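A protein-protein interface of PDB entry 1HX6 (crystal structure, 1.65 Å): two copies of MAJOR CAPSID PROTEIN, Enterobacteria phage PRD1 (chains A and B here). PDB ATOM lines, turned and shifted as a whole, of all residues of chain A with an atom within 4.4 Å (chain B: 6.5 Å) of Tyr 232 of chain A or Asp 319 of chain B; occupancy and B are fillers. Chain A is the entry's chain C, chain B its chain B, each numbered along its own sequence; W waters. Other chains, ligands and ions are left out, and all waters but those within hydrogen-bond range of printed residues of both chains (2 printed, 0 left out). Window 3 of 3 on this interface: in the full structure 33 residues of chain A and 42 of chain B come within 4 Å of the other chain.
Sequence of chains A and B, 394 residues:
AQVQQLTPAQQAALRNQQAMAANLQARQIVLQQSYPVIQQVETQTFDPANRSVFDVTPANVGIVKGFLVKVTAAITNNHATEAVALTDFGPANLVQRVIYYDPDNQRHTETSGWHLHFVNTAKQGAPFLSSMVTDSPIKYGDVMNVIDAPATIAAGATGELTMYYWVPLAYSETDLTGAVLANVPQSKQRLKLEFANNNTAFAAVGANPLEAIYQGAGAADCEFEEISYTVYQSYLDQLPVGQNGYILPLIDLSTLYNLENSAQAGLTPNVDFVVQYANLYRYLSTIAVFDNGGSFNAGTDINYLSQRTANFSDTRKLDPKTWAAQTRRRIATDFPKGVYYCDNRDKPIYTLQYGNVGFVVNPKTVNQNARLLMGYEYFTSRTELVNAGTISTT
O of Leu 68 of chain A sits at hydrogen-bond distance from N of Tyr 232 of chain A.
N of Lys 321 of chain B sits at hydrogen-bond distance from OD1 of Asp 319 of chain B.
O of Leu 305 of chain B is in hydrogen-bond range of N of Leu 318 of chain B.
The side-chain carboxylate of Asp 319 of chain B lies within hydrogen-bond range of the side-chain hydroxyl of Thr 322 of chain B (2.6 Å).
N of Lys 70 of chain A lies within hydrogen-bond range of O of Thr 230 of chain A (2.9 Å).
The side-chain carboxylate (OD1) of Asp 319 of chain B lies within salt-bridge range of the side-chain amino group (NZ) of Lys 70 of chain A (3.0 Å).
The side-chain hydroxyl (OH) of Tyr 164 of chain A is in hydrogen-bond range of the side-chain hydroxyl (OG1) of Thr 322 of chain B.
OD2 of Asp 319 of chain B lies within hydrogen-bond range of OH of Tyr 232 of chain A.
No position is printed for both chains.
Water W2 lies within hydrogen-bond range of O of Lys 317 of chain B (2.7 Å) and N of Gln 40 of chain A (2.9 Å).
Water W1 lies within hydrogen-bond range of the backbone carbonyl oxygen of Ile 38 of chain A and the backbone NH of Lys 317 of chain B.
Of the 12 printed residues of chain B, 5 touch a printed residue of chain A.
Hydrophobic or aromatic side chains of chain A within 4 Å of the printed part of chain B: Ile 38, Leu 68, Tyr 164 and Tyr 232.
Among the printed residues, 11 pairs touch across the chains.
Among the printed residues, Asp or Glu carboxylates within 4 Å of a Lys or Arg side-chain nitrogen of the other chain: Lys 70 of chain A with Asp 319 of chain B.
Of the printed residues of chain B, Tyr 232 of chain A touches Lys 317, Leu 318, Asp 319 and Thr 322.
Of the printed residues of chain B, Tyr 164 of chain A touches Asp 319 (3.97 Å), Lys 321 (3.3 Å) and Thr 322 (2.8 Å).
Of the printed residues of chain A, Lys 317 of chain B touches Tyr 232 (3.8 Å).
Printed residues of chain B within 4 Å of Lys 70 of chain A: Asp 319 and Thr 322.
Val 231 of chain A touches none of the printed residues of chain B.
Ile 302 of chain B touches none of the printed residues of chain A.
The nearest residue of chain B that does not touch Tyr 232 of chain A is Pro 320 of chain B (6.3 Å).
The nearest printed residue of chain A that does not touch Asp 319 of chain B is Thr 230 of chain A (5.1 Å).
The nearest printed residue of chain A that does not touch Leu 318 of chain B is Gln 39 of chain A (5.6 Å).
Ile 38 of chain A touches Leu 318 of chain B.
Thr 322 of chain B touches Leu 68 of chain A.
Thr 322 of chain B touches Lys 70 of chain A.
OH of Tyr 164 of chain A touches OD1 of Asp 319 of chain B, at 3.97 Å.
C of Lys 321 of chain B touches OH of Tyr 164 of chain A, at 3.3 Å.
Tyr 232 of chain A touches Lys 317 of chain B (CE1 to O, 3.8 Å).
Leu 318 of chain B touches Tyr 232 of chain A.
Tyr 232 of chain A touches Thr 322 of chain B.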
ATOM      1  N   ILE A  38      24.844  18.860   7.651  1.00  0.00           N
ATOM      2  CA  ILE A  38      25.934  18.668   8.592  1.00  0.00           C
ATOM      3  C   ILE A  38      26.760  17.579   7.928  1.00  0.00           C
ATOM      4  O   ILE A  38      26.242  16.511   7.609  1.00  0.00           O
ATOM      5  CB  ILE A  38      25.473  18.231  10.015  1.00  0.00           C
ATOM      6  CG1 ILE A  38      26.714  18.098  10.913  1.00  0.00           C
ATOM      7  CG2 ILE A  38      24.709  16.913   9.965  1.00  0.00           C
ATOM      8  CD1 ILE A  38      26.426  17.976  12.414  1.00  0.00           C
ATOM      9  N   GLN A  39      28.034  17.858   7.664  1.00  0.00           N
ATOM     10  CA  GLN A  39      28.861  16.853   7.014  1.00  0.00           C
ATOM     11  C   GLN A  39      30.297  16.860   7.500  1.00  0.00           C
ATOM     12  O   GLN A  39      30.831  17.905   7.874  1.00  0.00           O
ATOM     13  CB  GLN A  39      28.841  17.040   5.498  1.00  0.00           C
ATOM     14  CG  GLN A  39      29.624  18.206   4.990  1.00  0.00           C
ATOM     15  CD  GLN A  39      29.643  18.246   3.472  1.00  0.00           C
ATOM     16  OE1 GLN A  39      30.001  17.265   2.815  1.00  0.00           O
ATOM     17  NE2 GLN A  39      29.251  19.376   2.908  1.00  0.00           N
ATOM     18  N   GLN A  40      30.911  15.682   7.479  1.00  0.00           N
ATOM     19  CA  GLN A  40      32.282  15.532   7.930  1.00  0.00           C
ATOM     20  C   GLN A  40      33.229  16.341   7.062  1.00  0.00           C
ATOM     21  O   GLN A  40      33.111  16.342   5.831  1.00  0.00           O
ATOM     22  CB  GLN A  40      32.713  14.062   7.909  1.00  0.00           C
ATOM     23  CG  GLN A  40      34.164  13.876   8.342  1.00  0.00           C
ATOM     24  CD  GLN A  40      34.587  12.419   8.432  1.00  0.00           C
ATOM     25  OE1 GLN A  40      33.878  11.587   9.001  1.00  0.00           O
ATOM     26  NE2 GLN A  40      35.753  12.110   7.891  1.00  0.00           N
ATOM     27  N   GLY A  66      28.343  26.437  12.500  1.00  0.00           N
ATOM     28  CA  GLY A  66      29.224  25.957  13.556  1.00  0.00           C
ATOM     29  C   GLY A  66      29.830  24.605  13.236  1.00  0.00           C
ATOM     30  O   GLY A  66      29.611  24.039  12.160  1.00  0.00           O
ATOM     31  N   PHE A  67      30.597  24.077  14.184  1.00  0.00           N
ATOM     32  CA  PHE A  67      31.251  22.789  13.997  1.00  0.00           C
ATOM     33  C   PHE A  67      31.051  21.886  15.196  1.00  0.00           C
ATOM     34  O   PHE A  67      31.190  22.316  16.341  1.00  0.00           O
ATOM     35  CB  PHE A  67      32.761  22.971  13.785  1.00  0.00           C
ATOM     36  CG  PHE A  67      33.101  23.936  12.691  1.00  0.00           C
ATOM     37  CD1 PHE A  67      33.199  25.292  12.957  1.00  0.00           C
ATOM     38  CD2 PHE A  67      33.263  23.489  11.382  1.00  0.00           C
ATOM     39  CE1 PHE A  67      33.451  26.213  11.920  1.00  0.00           C
ATOM     40  CE2 PHE A  67      33.513  24.393  10.342  1.00  0.00           C
ATOM     41  CZ  PHE A  67      33.604  25.751  10.614  1.00  0.00           C
ATOM     42  N   LEU A  68      30.712  20.635  14.923  1.00  0.00           N
ATOM     43  CA  LEU A  68      30.556  19.656  15.990  1.00  0.00           C
ATOM     44  C   LEU A  68      31.849  18.845  15.916  1.00  0.00           C
ATOM     45  O   LEU A  68      32.164  18.254  14.893  1.00  0.00           O
ATOM     46  CB  LEU A  68      29.337  18.756  15.742  1.00  0.00           C
ATOM     47  CG  LEU A  68      29.050  17.732  16.862  1.00  0.00           C
ATOM     48  CD1 LEU A  68      28.744  18.457  18.187  1.00  0.00           C
ATOM     49  CD2 LEU A  68      27.866  16.844  16.452  1.00  0.00           C
ATOM     50  N   LYS A  70      33.945  15.726  17.389  1.00  0.00           N
ATOM     51  CA  LYS A  70      33.941  14.471  18.129  1.00  0.00           C
ATOM     52  C   LYS A  70      35.401  14.191  18.462  1.00  0.00           C
ATOM     53  O   LYS A  70      36.255  14.281  17.583  1.00  0.00           O
ATOM     54  CB  LYS A  70      33.405  13.341  17.247  1.00  0.00           C
ATOM     55  CG  LYS A  70      33.517  11.958  17.897  1.00  0.00           C
ATOM     56  CD  LYS A  70      33.088  10.871  16.932  1.00  0.00           C
ATOM     57  CE  LYS A  70      33.098   9.506  17.596  1.00  0.00           C
ATOM     58  NZ  LYS A  70      32.766   8.431  16.608  1.00  0.00           N
ATOM     59  N   TYR A 164      32.481  15.565  23.051  1.00  0.00           N
ATOM     60  CA  TYR A 164      31.983  16.372  21.931  1.00  0.00           C
ATOM     61  C   TYR A 164      31.975  17.832  22.320  1.00  0.00           C
ATOM     62  O   TYR A 164      31.673  18.171  23.468  1.00  0.00           O
ATOM     63  CB  TYR A 164      30.534  16.011  21.536  1.00  0.00           C
ATOM     64  CG  TYR A 164      30.403  14.789  20.668  1.00  0.00           C
ATOM     65  CD1 TYR A 164      30.440  13.505  21.223  1.00  0.00           C
ATOM     66  CD2 TYR A 164      30.250  14.910  19.285  1.00  0.00           C
ATOM     67  CE1 TYR A 164      30.332  12.379  20.420  1.00  0.00           C
ATOM     68  CE2 TYR A 164      30.140  13.788  18.470  1.00  0.00           C
ATOM     69  CZ  TYR A 164      30.182  12.527  19.048  1.00  0.00           C
ATOM     70  OH  TYR A 164      30.055  11.413  18.255  1.00  0.00           O
ATOM     71  N   THR A 230      37.034  14.087  14.741  1.00  0.00           N
ATOM     72  CA  THR A 230      36.274  14.150  13.508  1.00  0.00           C
ATOM     73  C   THR A 230      35.516  15.450  13.634  1.00  0.00           C
ATOM     74  O   THR A 230      34.791  15.676  14.616  1.00  0.00           O
ATOM     75  CB  THR A 230      35.266  12.994  13.353  1.00  0.00           C
ATOM     76  OG1 THR A 230      35.972  11.752  13.291  1.00  0.00           O
ATOM     77  CG2 THR A 230      34.480  13.154  12.054  1.00  0.00           C
ATOM     78  N   VAL A 231      35.694  16.314  12.645  1.00  0.00           N
ATOM     79  CA  VAL A 231      35.020  17.600  12.636  1.00  0.00           C
ATOM     80  C   VAL A 231      33.881  17.561  11.629  1.00  0.00           C
ATOM     81  O   VAL A 231      34.079  17.193  10.470  1.00  0.00           O
ATOM     82  CB  VAL A 231      35.988  18.748  12.220  1.00  0.00           C
ATOM     83  CG1 VAL A 231      35.185  20.071  12.063  1.00  0.00           C
ATOM     84  CG2 VAL A 231      37.110  18.914  13.271  1.00  0.00           C
ATOM     85  N   TYR A 232      32.685  17.921  12.088  1.00  0.00           N
ATOM     86  CA  TYR A 232      31.510  17.991  11.231  1.00  0.00           C
ATOM     87  C   TYR A 232      31.154  19.470  11.115  1.00  0.00           C
ATOM     88  O   TYR A 232      31.121  20.198  12.112  1.00  0.00           O
ATOM     89  CB  TYR A 232      30.321  17.229  11.841  1.00  0.00           C
ATOM     90  CG  TYR A 232      30.448  15.726  11.785  1.00  0.00           C
ATOM     91  CD1 TYR A 232      30.023  15.021  10.662  1.00  0.00           C
ATOM     92  CD2 TYR A 232      30.979  15.008  12.855  1.00  0.00           C
ATOM     93  CE1 TYR A 232      30.113  13.646  10.604  1.00  0.00           C
ATOM     94  CE2 TYR A 232      31.073  13.626  12.803  1.00  0.00           C
ATOM     95  CZ  TYR A 232      30.637  12.952  11.677  1.00  0.00           C
ATOM     96  OH  TYR A 232      30.714  11.576  11.620  1.00  0.00           O
ATOM     97  N   GLN A 233      30.888  19.916   9.892  1.00  0.00           N
ATOM     98  CA  GLN A 233      30.553  21.311   9.658  1.00  0.00           C
ATOM     99  C   GLN A 233      29.063  21.416   9.406  1.00  0.00           C
ATOM    100  O   GLN A 233      28.521  20.683   8.577  1.00  0.00           O
ATOM    101  CB  GLN A 233      31.316  21.835   8.437  1.00  0.00           C
ATOM    102  CG  GLN A 233      31.096  23.293   8.127  1.00  0.00           C
ATOM    103  CD  GLN A 233      32.014  23.769   7.015  1.00  0.00           C
ATOM    104  OE1 GLN A 233      33.187  23.392   6.959  1.00  0.00           O
ATOM    105  NE2 GLN A 233      31.493  24.597   6.133  1.00  0.00           N
ATOM    106  N   SER A 234      28.414  22.313  10.139  1.00  0.00           N
ATOM    107  CA  SER A 234      26.980  22.547  10.005  1.00  0.00           C
ATOM    108  C   SER A 234      26.788  23.846   9.228  1.00  0.00           C
ATOM    109  O   SER A 234      27.336  24.890   9.599  1.00  0.00           O
ATOM    110  CB  SER A 234      26.339  22.671  11.387  1.00  0.00           C
ATOM    111  OG  SER A 234      24.973  23.029  11.283  1.00  0.00           O
ATOM    112  N   ILE B 302      27.587  -0.689  12.688  1.00  0.00           N
ATOM    113  CA  ILE B 302      27.261   0.282  11.642  1.00  0.00           C
ATOM    114  C   ILE B 302      28.410   1.244  11.327  1.00  0.00           C
ATOM    115  O   ILE B 302      29.085   1.746  12.232  1.00  0.00           O
ATOM    116  CB  ILE B 302      26.013   1.130  12.046  1.00  0.00           C
ATOM    117  CG1 ILE B 302      24.774   0.231  12.108  1.00  0.00           C
ATOM    118  CG2 ILE B 302      25.780   2.267  11.030  1.00  0.00           C
ATOM    119  CD1 ILE B 302      23.529   0.956  12.561  1.00  0.00           C
ATOM    120  N   ASN B 303      28.636   1.506  10.042  1.00  0.00           N
ATOM    121  CA  ASN B 303      29.682   2.447   9.646  1.00  0.00           C
ATOM    122  C   ASN B 303      29.111   3.854   9.795  1.00  0.00           C
ATOM    123  O   ASN B 303      29.715   4.722  10.428  1.00  0.00           O
ATOM    124  CB  ASN B 303      30.108   2.217   8.189  1.00  0.00           C
ATOM    125  CG  ASN B 303      30.895   0.929   8.015  1.00  0.00           C
ATOM    126  OD1 ASN B 303      31.878   0.698   8.720  1.00  0.00           O
ATOM    127  ND2 ASN B 303      30.467   0.089   7.079  1.00  0.00           N
ATOM    128  N   TYR B 304      27.941   4.070   9.204  1.00  0.00           N
ATOM    129  CA  TYR B 304      27.268   5.361   9.290  1.00  0.00           C
ATOM    130  C   TYR B 304      25.812   5.265   8.872  1.00  0.00           C
ATOM    131  O   TYR B 304      25.390   4.262   8.295  1.00  0.00           O
ATOM    132  CB  TYR B 304      27.973   6.405   8.401  1.00  0.00           C
ATOM    133  CG  TYR B 304      28.036   6.062   6.916  1.00  0.00           C
ATOM    134  CD1 TYR B 304      26.937   6.252   6.075  1.00  0.00           C
ATOM    135  CD2 TYR B 304      29.216   5.577   6.350  1.00  0.00           C
ATOM    136  CE1 TYR B 304      27.021   5.967   4.686  1.00  0.00           C
ATOM    137  CE2 TYR B 304      29.307   5.290   4.984  1.00  0.00           C
ATOM    138  CZ  TYR B 304      28.215   5.488   4.161  1.00  0.00           C
ATOM    139  OH  TYR B 304      28.333   5.203   2.810  1.00  0.00           O
ATOM    140  N   LEU B 305      25.052   6.313   9.183  1.00  0.00           N
ATOM    141  CA  LEU B 305      23.647   6.412   8.802  1.00  0.00           C
ATOM    142  C   LEU B 305      23.530   7.755   8.098  1.00  0.00           C
ATOM    143  O   LEU B 305      24.350   8.653   8.321  1.00  0.00           O
ATOM    144  CB  LEU B 305      22.708   6.416  10.024  1.00  0.00           C
ATOM    145  CG  LEU B 305      22.744   5.210  10.968  1.00  0.00           C
ATOM    146  CD1 LEU B 305      23.725   5.469  12.118  1.00  0.00           C
ATOM    147  CD2 LEU B 305      21.335   4.972  11.534  1.00  0.00           C
ATOM    148  N   LYS B 317      25.116  12.660   6.900  1.00  0.00           N
ATOM    149  CA  LYS B 317      25.799  11.371   6.899  1.00  0.00           C
ATOM    150  C   LYS B 317      26.690  11.385   8.146  1.00  0.00           C
ATOM    151  O   LYS B 317      27.696  12.100   8.186  1.00  0.00           O
ATOM    152  CB  LYS B 317      26.642  11.251   5.642  1.00  0.00           C
ATOM    153  CG  LYS B 317      27.490   9.999   5.584  1.00  0.00           C
ATOM    154  CD  LYS B 317      28.352  10.034   4.325  1.00  0.00           C
ATOM    155  CE  LYS B 317      29.270   8.836   4.235  1.00  0.00           C
ATOM    156  NZ  LYS B 317      30.168   8.949   3.040  1.00  0.00           N
ATOM    157  N   LEU B 318      26.321  10.598   9.154  1.00  0.00           N
ATOM    158  CA  LEU B 318      27.042  10.597  10.426  1.00  0.00           C
ATOM    159  C   LEU B 318      27.430   9.231  10.967  1.00  0.00           C
ATOM    160  O   LEU B 318      26.739   8.235  10.713  1.00  0.00           O
ATOM    161  CB  LEU B 318      26.183  11.283  11.500  1.00  0.00           C
ATOM    162  CG  LEU B 318      25.566  12.651  11.207  1.00  0.00           C
ATOM    163  CD1 LEU B 318      24.559  13.032  12.302  1.00  0.00           C
ATOM    164  CD2 LEU B 318      26.678  13.694  11.116  1.00  0.00           C
ATOM    165  N   ASP B 319      28.521   9.198  11.736  1.00  0.00           N
ATOM    166  CA  ASP B 319      28.959   7.957  12.377  1.00  0.00           C
ATOM    167  C   ASP B 319      27.886   7.725  13.445  1.00  0.00           C
ATOM    168  O   ASP B 319      27.208   8.670  13.864  1.00  0.00           O
ATOM    169  CB  ASP B 319      30.364   8.114  13.008  1.00  0.00           C
ATOM    170  CG  ASP B 319      30.402   9.140  14.132  1.00  0.00           C
ATOM    171  OD1 ASP B 319      30.140   8.773  15.291  1.00  0.00           O
ATOM    172  OD2 ASP B 319      30.701  10.321  13.862  1.00  0.00           O
ATOM    173  N   PRO B 320      27.718   6.475  13.905  1.00  0.00           N
ATOM    174  CA  PRO B 320      26.688   6.199  14.914  1.00  0.00           C
ATOM    175  C   PRO B 320      26.671   7.043  16.192  1.00  0.00           C
ATOM    176  O   PRO B 320      25.602   7.426  16.655  1.00  0.00           O
ATOM    177  CB  PRO B 320      26.874   4.707  15.207  1.00  0.00           C
ATOM    178  CG  PRO B 320      27.399   4.170  13.877  1.00  0.00           C
ATOM    179  CD  PRO B 320      28.426   5.238  13.520  1.00  0.00           C
ATOM    180  N   LYS B 321      27.832   7.328  16.779  1.00  0.00           N
ATOM    181  CA  LYS B 321      27.818   8.124  18.004  1.00  0.00           C
ATOM    182  C   LYS B 321      27.395   9.565  17.752  1.00  0.00           C
ATOM    183  O   LYS B 321      26.715  10.170  18.583  1.00  0.00           O
ATOM    184  CB  LYS B 321      29.179   8.095  18.718  1.00  0.00           C
ATOM    185  CG  LYS B 321      29.368   6.903  19.669  1.00  0.00           C
ATOM    186  CD  LYS B 321      30.505   7.144  20.663  1.00  0.00           C
ATOM    187  CE  LYS B 321      30.772   5.912  21.533  1.00  0.00           C
ATOM    188  NZ  LYS B 321      31.747   6.185  22.635  1.00  0.00           N
ATOM    189  N   THR B 322      27.781  10.124  16.608  1.00  0.00           N
ATOM    190  CA  THR B 322      27.396  11.501  16.302  1.00  0.00           C
ATOM    191  C   THR B 322      25.896  11.553  15.981  1.00  0.00           C
ATOM    192  O   THR B 322      25.206  12.522  16.307  1.00  0.00           O
ATOM    193  CB  THR B 322      28.249  12.063  15.145  1.00  0.00           C
ATOM    194  OG1 THR B 322      29.624  12.053  15.550  1.00  0.00           O
ATOM    195  CG2 THR B 322      27.849  13.492  14.823  1.00  0.00           C
ATOM    196  N   TRP B 323      25.394  10.497  15.355  1.00  0.00           N
ATOM    197  CA  TRP B 323      23.967  10.402  15.073  1.00  0.00           C
ATOM    198  C   TRP B 323      23.254  10.358  16.437  1.00  0.00           C
ATOM    199  O   TRP B 323      22.270  11.069  16.681  1.00  0.00           O
ATOM    200  CB  TRP B 323      23.698   9.121  14.282  1.00  0.00           C
ATOM    201  CG  TRP B 323      22.278   8.947  13.887  1.00  0.00           C
ATOM    202  CD1 TRP B 323      21.244   8.506  14.675  1.00  0.00           C
ATOM    203  CD2 TRP B 323      21.717   9.230  12.606  1.00  0.00           C
ATOM    204  NE1 TRP B 323      20.073   8.502  13.954  1.00  0.00           N
ATOM    205  CE2 TRP B 323      20.337   8.942  12.681  1.00  0.00           C
ATOM    206  CE3 TRP B 323      22.248   9.706  11.396  1.00  0.00           C
ATOM    207  CZ2 TRP B 323      19.476   9.113  11.587  1.00  0.00           C
ATOM    208  CZ3 TRP B 323      21.395   9.879  10.312  1.00  0.00           C
ATOM    209  CH2 TRP B 323      20.024   9.581  10.417  1.00  0.00           C
ATOM    210  N   ALA B 324      23.776   9.532  17.336  1.00  0.00           N
ATOM    211  CA  ALA B 324      23.198   9.399  18.675  1.00  0.00           C
ATOM    212  C   ALA B 324      23.233  10.737  19.429  1.00  0.00           C
ATOM    213  O   ALA B 324      22.331  11.046  20.214  1.00  0.00           O
ATOM    214  CB  ALA B 324      23.961   8.309  19.457  1.00  0.00           C
HETATM  215  O   HOH W   1      26.264  14.874   5.070  1.00  0.00           O
HETATM  216  O   HOH W   2      29.305  13.515   6.479  1.00  0.00           O
